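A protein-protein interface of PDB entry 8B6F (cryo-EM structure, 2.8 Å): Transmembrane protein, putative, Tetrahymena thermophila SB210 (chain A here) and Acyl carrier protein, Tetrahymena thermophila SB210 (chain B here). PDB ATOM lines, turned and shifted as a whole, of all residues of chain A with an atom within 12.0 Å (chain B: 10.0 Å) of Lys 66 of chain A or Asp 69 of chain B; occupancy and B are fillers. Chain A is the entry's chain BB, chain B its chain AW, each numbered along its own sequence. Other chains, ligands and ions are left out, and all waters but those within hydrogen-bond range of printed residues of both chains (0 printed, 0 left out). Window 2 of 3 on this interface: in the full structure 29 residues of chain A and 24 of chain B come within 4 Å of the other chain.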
ATOM      1  N   ILE A  60      -3.595 -12.310  30.028  1.00  0.00           N
ATOM      2  CA  ILE A  60      -4.810 -12.158  29.233  1.00  0.00           C
ATOM      3  C   ILE A  60      -4.988 -13.421  28.405  1.00  0.00           C
ATOM      4  O   ILE A  60      -4.074 -13.829  27.679  1.00  0.00           O
ATOM      5  CB  ILE A  60      -4.756 -10.907  28.330  1.00  0.00           C
ATOM      6  CG1 ILE A  60      -5.010  -9.616  29.122  1.00  0.00           C
ATOM      7  CG2 ILE A  60      -5.764 -11.001  27.188  1.00  0.00           C
ATOM      8  CD1 ILE A  60      -3.968  -9.258  30.149  1.00  0.00           C
ATOM      9  N   GLY A  61      -6.164 -14.034  28.511  1.00  0.00           N
ATOM     10  CA  GLY A  61      -6.463 -15.283  27.844  1.00  0.00           C
ATOM     11  C   GLY A  61      -6.982 -15.171  26.431  1.00  0.00           C
ATOM     12  O   GLY A  61      -7.247 -16.199  25.800  1.00  0.00           O
ATOM     13  N   ASN A  62      -7.142 -13.960  25.907  1.00  0.00           N
ATOM     14  CA  ASN A  62      -7.673 -13.789  24.562  1.00  0.00           C
ATOM     15  C   ASN A  62      -6.615 -14.149  23.529  1.00  0.00           C
ATOM     16  O   ASN A  62      -5.465 -13.710  23.624  1.00  0.00           O
ATOM     17  CB  ASN A  62      -8.149 -12.353  24.359  1.00  0.00           C
ATOM     18  CG  ASN A  62      -9.239 -11.962  25.332  1.00  0.00           C
ATOM     19  OD1 ASN A  62      -9.039 -11.106  26.192  1.00  0.00           O
ATOM     20  ND2 ASN A  62     -10.402 -12.590  25.203  1.00  0.00           N
ATOM     21  N   LYS A  63      -7.008 -14.948  22.537  1.00  0.00           N
ATOM     22  CA  LYS A  63      -6.064 -15.359  21.503  1.00  0.00           C
ATOM     23  C   LYS A  63      -5.742 -14.211  20.555  1.00  0.00           C
ATOM     24  O   LYS A  63      -4.609 -14.097  20.075  1.00  0.00           O
ATOM     25  CB  LYS A  63      -6.625 -16.552  20.730  1.00  0.00           C
ATOM     26  CG  LYS A  63      -6.813 -17.806  21.570  1.00  0.00           C
ATOM     27  CD  LYS A  63      -5.477 -18.386  22.013  1.00  0.00           C
ATOM     28  CE  LYS A  63      -5.667 -19.643  22.843  1.00  0.00           C
ATOM     29  NZ  LYS A  63      -6.419 -19.374  24.100  1.00  0.00           N
ATOM     30  N   SER A  64      -6.721 -13.359  20.264  1.00  0.00           N
ATOM     31  CA  SER A  64      -6.500 -12.222  19.382  1.00  0.00           C
ATOM     32  C   SER A  64      -7.575 -11.179  19.643  1.00  0.00           C
ATOM     33  O   SER A  64      -8.659 -11.488  20.145  1.00  0.00           O
ATOM     34  CB  SER A  64      -6.498 -12.643  17.910  1.00  0.00           C
ATOM     35  OG  SER A  64      -7.743 -13.200  17.540  1.00  0.00           O
ATOM     36  N   PHE A  65      -7.258  -9.932  19.292  1.00  0.00           N
ATOM     37  CA  PHE A  65      -8.200  -8.837  19.485  1.00  0.00           C
ATOM     38  C   PHE A  65      -9.296  -8.825  18.426  1.00  0.00           C
ATOM     39  O   PHE A  65     -10.434  -8.454  18.728  1.00  0.00           O
ATOM     40  CB  PHE A  65      -7.462  -7.497  19.478  1.00  0.00           C
ATOM     41  CG  PHE A  65      -8.330  -6.326  19.840  1.00  0.00           C
ATOM     42  CD1 PHE A  65      -9.089  -5.682  18.877  1.00  0.00           C
ATOM     43  CD2 PHE A  65      -8.384  -5.868  21.144  1.00  0.00           C
ATOM     44  CE1 PHE A  65      -9.887  -4.605  19.211  1.00  0.00           C
ATOM     45  CE2 PHE A  65      -9.181  -4.793  21.484  1.00  0.00           C
ATOM     46  CZ  PHE A  65      -9.932  -4.160  20.518  1.00  0.00           C
ATOM     47  N   LYS A  66      -8.979  -9.209  17.189  1.00  0.00           N
ATOM     48  CA  LYS A  66      -9.966  -9.141  16.116  1.00  0.00           C
ATOM     49  C   LYS A  66     -10.940 -10.312  16.180  1.00  0.00           C
ATOM     50  O   LYS A  66     -12.159 -10.114  16.159  1.00  0.00           O
ATOM     51  CB  LYS A  66      -9.263  -9.107  14.757  1.00  0.00           C
ATOM     52  CG  LYS A  66      -8.702  -7.745  14.365  1.00  0.00           C
ATOM     53  CD  LYS A  66      -7.585  -7.299  15.298  1.00  0.00           C
ATOM     54  CE  LYS A  66      -6.892  -6.051  14.771  1.00  0.00           C
ATOM     55  NZ  LYS A  66      -5.852  -5.551  15.716  1.00  0.00           N
ATOM     56  N   ASP A  67     -10.420 -11.540  16.260  1.00  0.00           N
ATOM     57  CA  ASP A  67     -11.293 -12.710  16.241  1.00  0.00           C
ATOM     58  C   ASP A  67     -12.251 -12.702  17.425  1.00  0.00           C
ATOM     59  O   ASP A  67     -13.440 -13.006  17.273  1.00  0.00           O
ATOM     60  CB  ASP A  67     -10.458 -13.989  16.230  1.00  0.00           C
ATOM     61  CG  ASP A  67      -9.423 -13.997  15.125  1.00  0.00           C
ATOM     62  OD1 ASP A  67      -9.654 -13.338  14.090  1.00  0.00           O
ATOM     63  OD2 ASP A  67      -8.375 -14.655  15.291  1.00  0.00           O
ATOM     64  N   ASP A  68     -11.754 -12.367  18.610  1.00  0.00           N
ATOM     65  CA  ASP A  68     -12.598 -12.200  19.784  1.00  0.00           C
ATOM     66  C   ASP A  68     -13.074 -10.757  19.844  1.00  0.00           C
ATOM     67  O   ASP A  68     -12.277  -9.828  19.682  1.00  0.00           O
ATOM     68  CB  ASP A  68     -11.834 -12.554  21.060  1.00  0.00           C
ATOM     69  CG  ASP A  68     -11.075 -13.857  20.944  1.00  0.00           C
ATOM     70  OD1 ASP A  68     -11.503 -14.725  20.156  1.00  0.00           O
ATOM     71  OD2 ASP A  68     -10.049 -14.011  21.637  1.00  0.00           O
ATOM     72  N   LEU A  69     -14.368 -10.566  20.081  1.00  0.00           N
ATOM     73  CA  LEU A  69     -14.922  -9.221  20.113  1.00  0.00           C
ATOM     74  C   LEU A  69     -14.505  -8.516  21.396  1.00  0.00           C
ATOM     75  O   LEU A  69     -15.341  -8.223  22.255  1.00  0.00           O
ATOM     76  CB  LEU A  69     -16.445  -9.264  19.987  1.00  0.00           C
ATOM     77  CG  LEU A  69     -16.983  -9.854  18.682  1.00  0.00           C
ATOM     78  CD1 LEU A  69     -18.498  -9.856  18.689  1.00  0.00           C
ATOM     79  CD2 LEU A  69     -16.463  -9.095  17.469  1.00  0.00           C
ATOM     80  N   VAL A  70     -13.207  -8.242  21.525  1.00  0.00           N
ATOM     81  CA  VAL A  70     -12.703  -7.568  22.716  1.00  0.00           C
ATOM     82  C   VAL A  70     -13.326  -6.187  22.846  1.00  0.00           C
ATOM     83  O   VAL A  70     -13.653  -5.738  23.951  1.00  0.00           O
ATOM     84  CB  VAL A  70     -11.164  -7.494  22.671  1.00  0.00           C
ATOM     85  CG1 VAL A  70     -10.629  -6.635  23.806  1.00  0.00           C
ATOM     86  CG2 VAL A  70     -10.565  -8.889  22.729  1.00  0.00           C
ATOM     87  N   ALA A  71     -13.503  -5.491  21.723  1.00  0.00           N
ATOM     88  CA  ALA A  71     -14.092  -4.160  21.765  1.00  0.00           C
ATOM     89  C   ALA A  71     -15.491  -4.173  22.362  1.00  0.00           C
ATOM     90  O   ALA A  71     -15.963  -3.130  22.828  1.00  0.00           O
ATOM     91  CB  ALA A  71     -14.131  -3.561  20.360  1.00  0.00           C
ATOM     92  N   VAL A  72     -16.162  -5.320  22.358  1.00  0.00           N
ATOM     93  CA  VAL A  72     -17.492  -5.446  22.933  1.00  0.00           C
ATOM     94  C   VAL A  72     -17.447  -6.091  24.312  1.00  0.00           C
ATOM     95  O   VAL A  72     -18.109  -5.621  25.238  1.00  0.00           O
ATOM     96  CB  VAL A  72     -18.409  -6.243  21.979  1.00  0.00           C
ATOM     97  CG1 VAL A  72     -19.822  -6.327  22.537  1.00  0.00           C
ATOM     98  CG2 VAL A  72     -18.418  -5.610  20.596  1.00  0.00           C
ATOM     99  N   TYR A  73     -16.673  -7.165  24.467  1.00  0.00           N
ATOM    100  CA  TYR A  73     -16.632  -7.918  25.714  1.00  0.00           C
ATOM    101  C   TYR A  73     -15.373  -7.669  26.533  1.00  0.00           C
ATOM    102  O   TYR A  73     -15.272  -8.185  27.651  1.00  0.00           O
ATOM    103  CB  TYR A  73     -16.748  -9.417  25.421  1.00  0.00           C
ATOM    104  CG  TYR A  73     -17.976  -9.783  24.623  1.00  0.00           C
ATOM    105  CD1 TYR A  73     -19.188 -10.031  25.250  1.00  0.00           C
ATOM    106  CD2 TYR A  73     -17.922  -9.878  23.241  1.00  0.00           C
ATOM    107  CE1 TYR A  73     -20.313 -10.364  24.523  1.00  0.00           C
ATOM    108  CE2 TYR A  73     -19.040 -10.210  22.504  1.00  0.00           C
ATOM    109  CZ  TYR A  73     -20.233 -10.452  23.151  1.00  0.00           C
ATOM    110  OH  TYR A  73     -21.350 -10.784  22.421  1.00  0.00           O
ATOM    111  N   GLY A  74     -14.417  -6.906  26.017  1.00  0.00           N
ATOM    112  CA  GLY A  74     -13.212  -6.625  26.767  1.00  0.00           C
ATOM    113  C   GLY A  74     -12.268  -7.818  26.813  1.00  0.00           C
ATOM    114  O   GLY A  74     -12.424  -8.813  26.107  1.00  0.00           O
ATOM    115  N   PHE A  75     -11.266  -7.689  27.676  1.00  0.00           N
ATOM    116  CA  PHE A  75     -10.237  -8.704  27.846  1.00  0.00           C
ATOM    117  C   PHE A  75     -10.581  -9.614  29.017  1.00  0.00           C
ATOM    118  O   PHE A  75     -11.050  -9.152  30.059  1.00  0.00           O
ATOM    119  CB  PHE A  75      -8.870  -8.062  28.091  1.00  0.00           C
ATOM    120  CG  PHE A  75      -8.310  -7.345  26.900  1.00  0.00           C
ATOM    121  CD1 PHE A  75      -7.656  -8.043  25.899  1.00  0.00           C
ATOM    122  CD2 PHE A  75      -8.410  -5.969  26.796  1.00  0.00           C
ATOM    123  CE1 PHE A  75      -7.129  -7.383  24.806  1.00  0.00           C
ATOM    124  CE2 PHE A  75      -7.885  -5.302  25.706  1.00  0.00           C
ATOM    125  CZ  PHE A  75      -7.242  -6.011  24.710  1.00  0.00           C
ATOM    126  N   THR A  76     -10.346 -10.911  28.838  1.00  0.00           N
ATOM    127  CA  THR A  76     -10.487 -11.877  29.916  1.00  0.00           C
ATOM    128  C   THR A  76      -9.186 -11.972  30.703  1.00  0.00           C
ATOM    129  O   THR A  76      -8.094 -11.794  30.158  1.00  0.00           O
ATOM    130  CB  THR A  76     -10.866 -13.258  29.375  1.00  0.00           C
ATOM    131  OG1 THR A  76      -9.876 -13.700  28.437  1.00  0.00           O
ATOM    132  CG2 THR A  76     -12.224 -13.211  28.696  1.00  0.00           C
ATOM    133  N   ARG B  63      -2.982  -4.922  28.588  1.00  0.00           N
ATOM    134  CA  ARG B  63      -4.168  -4.576  27.813  1.00  0.00           C
ATOM    135  C   ARG B  63      -3.859  -3.457  26.831  1.00  0.00           C
ATOM    136  O   ARG B  63      -4.276  -3.508  25.669  1.00  0.00           O
ATOM    137  CB  ARG B  63      -5.312  -4.166  28.741  1.00  0.00           C
ATOM    138  CG  ARG B  63      -5.844  -5.285  29.620  1.00  0.00           C
ATOM    139  CD  ARG B  63      -7.125  -4.859  30.323  1.00  0.00           C
ATOM    140  NE  ARG B  63      -7.477  -5.749  31.424  1.00  0.00           N
ATOM    141  CZ  ARG B  63      -7.168  -5.538  32.696  1.00  0.00           C
ATOM    142  NH1 ARG B  63      -6.497  -4.465  33.079  1.00  0.00           N
ATOM    143  NH2 ARG B  63      -7.547  -6.427  33.610  1.00  0.00           N
ATOM    144  N   LEU B  64      -3.126  -2.438  27.276  1.00  0.00           N
ATOM    145  CA  LEU B  64      -2.758  -1.352  26.376  1.00  0.00           C
ATOM    146  C   LEU B  64      -1.926  -1.872  25.213  1.00  0.00           C
ATOM    147  O   LEU B  64      -2.134  -1.473  24.061  1.00  0.00           O
ATOM    148  CB  LEU B  64      -1.994  -0.275  27.143  1.00  0.00           C
ATOM    149  CG  LEU B  64      -1.563   0.944  26.326  1.00  0.00           C
ATOM    150  CD1 LEU B  64      -2.768   1.722  25.828  1.00  0.00           C
ATOM    151  CD2 LEU B  64      -0.660   1.830  27.154  1.00  0.00           C
ATOM    152  N   ILE B  65      -0.973  -2.762  25.496  1.00  0.00           N
ATOM    153  CA  ILE B  65      -0.150  -3.337  24.437  1.00  0.00           C
ATOM    154  C   ILE B  65      -1.011  -4.141  23.473  1.00  0.00           C
ATOM    155  O   ILE B  65      -0.858  -4.043  22.250  1.00  0.00           O
ATOM    156  CB  ILE B  65       0.979  -4.195  25.041  1.00  0.00           C
ATOM    157  CG1 ILE B  65       1.952  -3.316  25.826  1.00  0.00           C
ATOM    158  CG2 ILE B  65       1.731  -4.948  23.953  1.00  0.00           C
ATOM    159  CD1 ILE B  65       2.861  -4.094  26.748  1.00  0.00           C
ATOM    160  N   SER B  66      -1.935  -4.943  24.004  1.00  0.00           N
ATOM    161  CA  SER B  66      -2.789  -5.752  23.142  1.00  0.00           C
ATOM    162  C   SER B  66      -3.673  -4.889  22.253  1.00  0.00           C
ATOM    163  O   SER B  66      -4.028  -5.305  21.144  1.00  0.00           O
ATOM    164  CB  SER B  66      -3.654  -6.678  23.995  1.00  0.00           C
ATOM    165  OG  SER B  66      -2.850  -7.507  24.814  1.00  0.00           O
ATOM    166  N   LEU B  67      -4.044  -3.695  22.715  1.00  0.00           N
ATOM    167  CA  LEU B  67      -4.861  -2.809  21.893  1.00  0.00           C
ATOM    168  C   LEU B  67      -4.171  -2.456  20.581  1.00  0.00           C
ATOM    169  O   LEU B  67      -4.847  -2.150  19.592  1.00  0.00           O
ATOM    170  CB  LEU B  67      -5.195  -1.533  22.668  1.00  0.00           C
ATOM    171  CG  LEU B  67      -6.226  -1.652  23.792  1.00  0.00           C
ATOM    172  CD1 LEU B  67      -6.392  -0.319  24.498  1.00  0.00           C
ATOM    173  CD2 LEU B  67      -7.565  -2.146  23.277  1.00  0.00           C
ATOM    174  N   HIS B  68      -2.843  -2.495  20.547  1.00  0.00           N
ATOM    175  CA  HIS B  68      -2.113  -2.079  19.358  1.00  0.00           C
ATOM    176  C   HIS B  68      -2.374  -3.034  18.198  1.00  0.00           C
ATOM    177  O   HIS B  68      -2.675  -4.214  18.388  1.00  0.00           O
ATOM    178  CB  HIS B  68      -0.615  -2.009  19.652  1.00  0.00           C
ATOM    179  CG  HIS B  68       0.136  -1.091  18.738  1.00  0.00           C
ATOM    180  ND1 HIS B  68       0.512  -1.451  17.463  1.00  0.00           N
ATOM    181  CD2 HIS B  68       0.584   0.174  18.918  1.00  0.00           C
ATOM    182  CE1 HIS B  68       1.156  -0.448  16.896  1.00  0.00           C
ATOM    183  NE2 HIS B  68       1.214   0.551  17.757  1.00  0.00           N
ATOM    184  N   ASP B  69      -2.256  -2.502  16.979  1.00  0.00           N
ATOM    185  CA  ASP B  69      -2.545  -3.297  15.789  1.00  0.00           C
ATOM    186  C   ASP B  69      -1.453  -4.325  15.521  1.00  0.00           C
ATOM    187  O   ASP B  69      -1.747  -5.469  15.157  1.00  0.00           O
ATOM    188  CB  ASP B  69      -2.715  -2.379  14.581  1.00  0.00           C
ATOM    189  CG  ASP B  69      -3.838  -1.380  14.763  1.00  0.00           C
ATOM    190  OD1 ASP B  69      -4.837  -1.725  15.425  1.00  0.00           O
ATOM    191  OD2 ASP B  69      -3.721  -0.249  14.250  1.00  0.00           O
ATOM    192  N   LYS B  70      -0.187  -3.935  15.686  1.00  0.00           N
ATOM    193  CA  LYS B  70       0.910  -4.856  15.409  1.00  0.00           C
ATOM    194  C   LYS B  70       0.863  -6.075  16.318  1.00  0.00           C
ATOM    195  O   LYS B  70       1.232  -7.176  15.895  1.00  0.00           O
ATOM    196  CB  LYS B  70       2.249  -4.135  15.559  1.00  0.00           C
ATOM    197  CG  LYS B  70       2.459  -3.004  14.563  1.00  0.00           C
ATOM    198  CD  LYS B  70       2.568  -3.523  13.137  1.00  0.00           C
ATOM    199  CE  LYS B  70       2.862  -2.394  12.163  1.00  0.00           C
ATOM    200  NZ  LYS B  70       3.012  -2.890  10.766  1.00  0.00           N
ATOM    201  N   VAL B  71       0.421  -5.903  17.562  1.00  0.00           N
ATOM    202  CA  VAL B  71       0.317  -7.028  18.480  1.00  0.00           C
ATOM    203  C   VAL B  71      -0.753  -7.984  17.976  1.00  0.00           C
ATOM    204  O   VAL B  71      -1.890  -7.580  17.698  1.00  0.00           O
ATOM    205  CB  VAL B  71       0.008  -6.532  19.901  1.00  0.00           C
ATOM    206  CG1 VAL B  71      -0.188  -7.703  20.854  1.00  0.00           C
ATOM    207  CG2 VAL B  71       1.123  -5.626  20.390  1.00  0.00           C
ATOM    208  N   GLN B  72      -0.394  -9.261  17.855  1.00  0.00           N
ATOM    209  CA  GLN B  72      -1.274 -10.274  17.287  1.00  0.00           C
ATOM    210  C   GLN B  72      -1.914 -11.163  18.346  1.00  0.00           C
ATOM    211  O   GLN B  72      -3.139 -11.306  18.374  1.00  0.00           O
ATOM    212  CB  GLN B  72      -0.492 -11.141  16.291  1.00  0.00           C
ATOM    213  CG  GLN B  72       0.168 -10.354  15.169  1.00  0.00           C
ATOM    214  CD  GLN B  72      -0.834  -9.629  14.295  1.00  0.00           C
ATOM    215  OE1 GLN B  72      -2.028  -9.927  14.320  1.00  0.00           O
ATOM    216  NE2 GLN B  72      -0.351  -8.669  13.515  1.00  0.00           N
ATOM    217  N   ASN B  73      -1.108 -11.764  19.221  1.00  0.00           N
ATOM    218  CA  ASN B  73      -1.607 -12.701  20.221  1.00  0.00           C
ATOM    219  C   ASN B  73      -1.435 -12.117  21.616  1.00  0.00           C
ATOM    220  O   ASN B  73      -0.317 -12.115  22.154  1.00  0.00           O
ATOM    221  CB  ASN B  73      -0.870 -14.039  20.112  1.00  0.00           C
ATOM    222  CG  ASN B  73      -1.499 -15.120  20.966  1.00  0.00           C
ATOM    223  OD1 ASN B  73      -2.370 -14.845  21.790  1.00  0.00           O
ATOM    224  ND2 ASN B  73      -1.056 -16.357  20.778  1.00  0.00           N
ATOM    225  N   PRO B  74      -2.495 -11.605  22.245  1.00  0.00           N
ATOM    226  CA  PRO B  74      -2.358 -11.141  23.635  1.00  0.00           C
ATOM    227  C   PRO B  74      -1.931 -12.233  24.597  1.00  0.00           C
ATOM    228  O   PRO B  74      -1.311 -11.932  25.623  1.00  0.00           O
ATOM    229  CB  PRO B  74      -3.761 -10.612  23.967  1.00  0.00           C
ATOM    230  CG  PRO B  74      -4.363 -10.278  22.652  1.00  0.00           C
ATOM    231  CD  PRO B  74      -3.822 -11.288  21.688  1.00  0.00           C
ATOM    232  N   ILE B  86       7.276 -10.025  21.295  1.00  0.00           N
ATOM    233  CA  ILE B  86       5.828  -9.848  21.337  1.00  0.00           C
ATOM    234  C   ILE B  86       5.330  -9.095  20.110  1.00  0.00           C
ATOM    235  O   ILE B  86       4.126  -9.091  19.838  1.00  0.00           O
ATOM    236  CB  ILE B  86       5.372  -9.129  22.621  1.00  0.00           C
ATOM    237  CG1 ILE B  86       5.932  -7.705  22.669  1.00  0.00           C
ATOM    238  CG2 ILE B  86       5.794  -9.932  23.841  1.00  0.00           C
ATOM    239  CD1 ILE B  86       5.590  -6.940  23.932  1.00  0.00           C
ATOM    240  N   GLY B  87       6.226  -8.450  19.365  1.00  0.00           N
ATOM    241  CA  GLY B  87       5.880  -7.825  18.107  1.00  0.00           C
ATOM    242  C   GLY B  87       5.876  -6.310  18.103  1.00  0.00           C
ATOM    243  O   GLY B  87       5.426  -5.717  17.117  1.00  0.00           O
ATOM    244  N   VAL B  88       6.362  -5.666  19.160  1.00  0.00           N
ATOM    245  CA  VAL B  88       6.378  -4.209  19.233  1.00  0.00           C
ATOM    246  C   VAL B  88       7.636  -3.710  18.527  1.00  0.00           C
ATOM    247  O   VAL B  88       8.755  -3.956  18.979  1.00  0.00           O
ATOM    248  CB  VAL B  88       6.322  -3.720  20.686  1.00  0.00           C
ATOM    249  CG1 VAL B  88       6.487  -2.207  20.756  1.00  0.00           C
ATOM    250  CG2 VAL B  88       5.015  -4.140  21.334  1.00  0.00           C
ATOM    251  N   ASP B  89       7.448  -3.007  17.413  1.00  0.00           N
ATOM    252  CA  ASP B  89       8.558  -2.421  16.686  1.00  0.00           C
ATOM    253  C   ASP B  89       9.137  -1.247  17.471  1.00  0.00           C
ATOM    254  O   ASP B  89       8.491  -0.717  18.378  1.00  0.00           O
ATOM    255  CB  ASP B  89       8.099  -1.953  15.308  1.00  0.00           C
ATOM    256  CG  ASP B  89       7.700  -3.103  14.406  1.00  0.00           C
ATOM    257  OD1 ASP B  89       8.355  -4.165  14.470  1.00  0.00           O
ATOM    258  OD2 ASP B  89       6.729  -2.948  13.637  1.00  0.00           O
ATOM    259  N   SER B  92       6.661   1.543  17.100  1.00  0.00           N
ATOM    260  CA  SER B  92       5.423   1.267  17.819  1.00  0.00           C
ATOM    261  C   SER B  92       5.626   1.380  19.322  1.00  0.00           C
ATOM    262  O   SER B  92       4.676   1.663  20.059  1.00  0.00           O
ATOM    263  CB  SER B  92       4.901  -0.123  17.462  1.00  0.00           C
ATOM    264  OG  SER B  92       4.666  -0.237  16.071  1.00  0.00           O
ATOM    265  N   GLU B  95       4.842   4.934  20.628  1.00  0.00           N
ATOM    266  CA  GLU B  95       3.402   5.173  20.673  1.00  0.00           C
ATOM    267  C   GLU B  95       2.776   4.486  21.878  1.00  0.00           C
ATOM    268  O   GLU B  95       1.982   5.086  22.609  1.00  0.00           O
ATOM    269  CB  GLU B  95       2.748   4.677  19.384  1.00  0.00           C
ATOM    270  CG  GLU B  95       3.354   5.244  18.118  1.00  0.00           C
ATOM    271  CD  GLU B  95       2.846   4.542  16.877  1.00  0.00           C
ATOM    272  OE1 GLU B  95       2.001   3.634  17.014  1.00  0.00           O
ATOM    273  OE2 GLU B  95       3.293   4.894  15.766  1.00  0.00           O
ATOM    274  N   ILE B  96       3.122   3.216  22.095  1.00  0.00           N
ATOM    275  CA  ILE B  96       2.563   2.477  23.222  1.00  0.00           C
ATOM    276  C   ILE B  96       2.966   3.130  24.535  1.00  0.00           C
ATOM    277  O   ILE B  96       2.179   3.184  25.488  1.00  0.00           O
ATOM    278  CB  ILE B  96       3.001   1.002  23.158  1.00  0.00           C
ATOM    279  CG1 ILE B  96       2.397   0.331  21.922  1.00  0.00           C
ATOM    280  CG2 ILE B  96       2.588   0.263  24.426  1.00  0.00           C
ATOM    281  CD1 ILE B  96       2.924  -1.063  21.651  1.00  0.00           C
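The side-chain amino group (NZ) of Lys 66 of chain A lies within salt-bridge range of the side-chain carboxylate (OD1) of Asp 69 of chain B (3.97 Å). OD1 of Asn 73 of chain B lies close to O of Lys 63 of chain A (2.9 Å).
The side-chain amide nitrogen of Gln 72 of chain B lies within hydrogen-bond range of the backbone carbonyl oxygen of Lys 70 of chain B, 3.2 Å away. N of Thr 76 of chain A lies within hydrogen-bond range of OD1 of Asn 62 of chain A, 3.0 Å away. The backbone NH (N) of Lys 63 of chain A sits at hydrogen-bond distance from the side-chain carboxylate (OD2) of Asp 68 of chain A. The side-chain hydroxyl of Ser 64 of chain A is in hydrogen-bond range of the side-chain carboxylate of Asp 67 of chain A, at 2.8 Å.
Lys 66 of chain A touches just one residue of chain B: Asp 69. His 68 of chain B touches none of the printed residues of chain A. Lys 70 of chain B touches none of the printed residues of chain A. No residue of chain A comes within 4 Å of Val 71 of chain B. Of chain A, only Lys 63 (3.6 Å) and Ser 64 (3.6 Å) come within 4 Å of Gln 72 of chain B. Of the printed residues of chain A, Leu 67 of chain B touches Phe 65 (3.6 Å) and Phe 75 (3.995 Å). Of the printed residues of chain A, Ser 66 of chain B touches Phe 75. Printed residues of chain A within 4 Å of Arg 63 of chain B: Phe 75. Printed residues of chain B within 4 Å of Lys 63 of chain A: Gln 72, Asn 73 and Pro 74. Printed residues of chain A within 4 Å of Pro 74 of chain B: Ile 60, Asn 62, Lys 63 and Ser 64. Tyr 73 of chain A touches none of the printed residues of chain B. Val 70 of chain A touches none of the printed residues of chain B. The nearest printed residue of chain B that does not touch Phe 75 of chain A is Pro 74 of chain B (4.5 Å).
Of the 17 printed residues of chain A, 7 touch a printed residue of chain B. Hydrophobic or aromatic side chains of chain A within 4 Å of the printed part of chain B: Ile 60, Phe 65 and Phe 75. Printed residues of chain B that touch a printed residue of chain A: Arg 63, Ser 66, Leu 67, Asp 69, Gln 72, Asn 73 and Pro 74. Hydrophobic or aromatic side chains of chain B that line the printed part of chain A: Leu 67 and Pro 74.
Among the printed residues, merely in contact across the chains: Lys 63 of chain A with Pro 74 of chain B (3.3 Å), Asn 62 of chain A with Pro 74 of chain B (3.5 Å), Phe 65 of chain A with Leu 67 of chain B (3.6 Å), Lys 63 of chain A with Gln 72 of chain B (3.6 Å), Ser 64 of chain A with Gln 72 of chain B (3.6 Å), Phe 75 of chain A with Ser 66 of chain B (3.6 Å), Ser 64 of chain A with Pro 74 of chain B (3.7 Å), Asn 62 of chain A with Asn 73 of chain B (3.8 Å), Ile 60 of chain A with Pro 74 of chain B (3.8 Å), Phe 75 of chain A with Arg 63 of chain B (3.9 Å) and Phe 75 of chain A with Leu 67 of chain B (3.995 Å).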
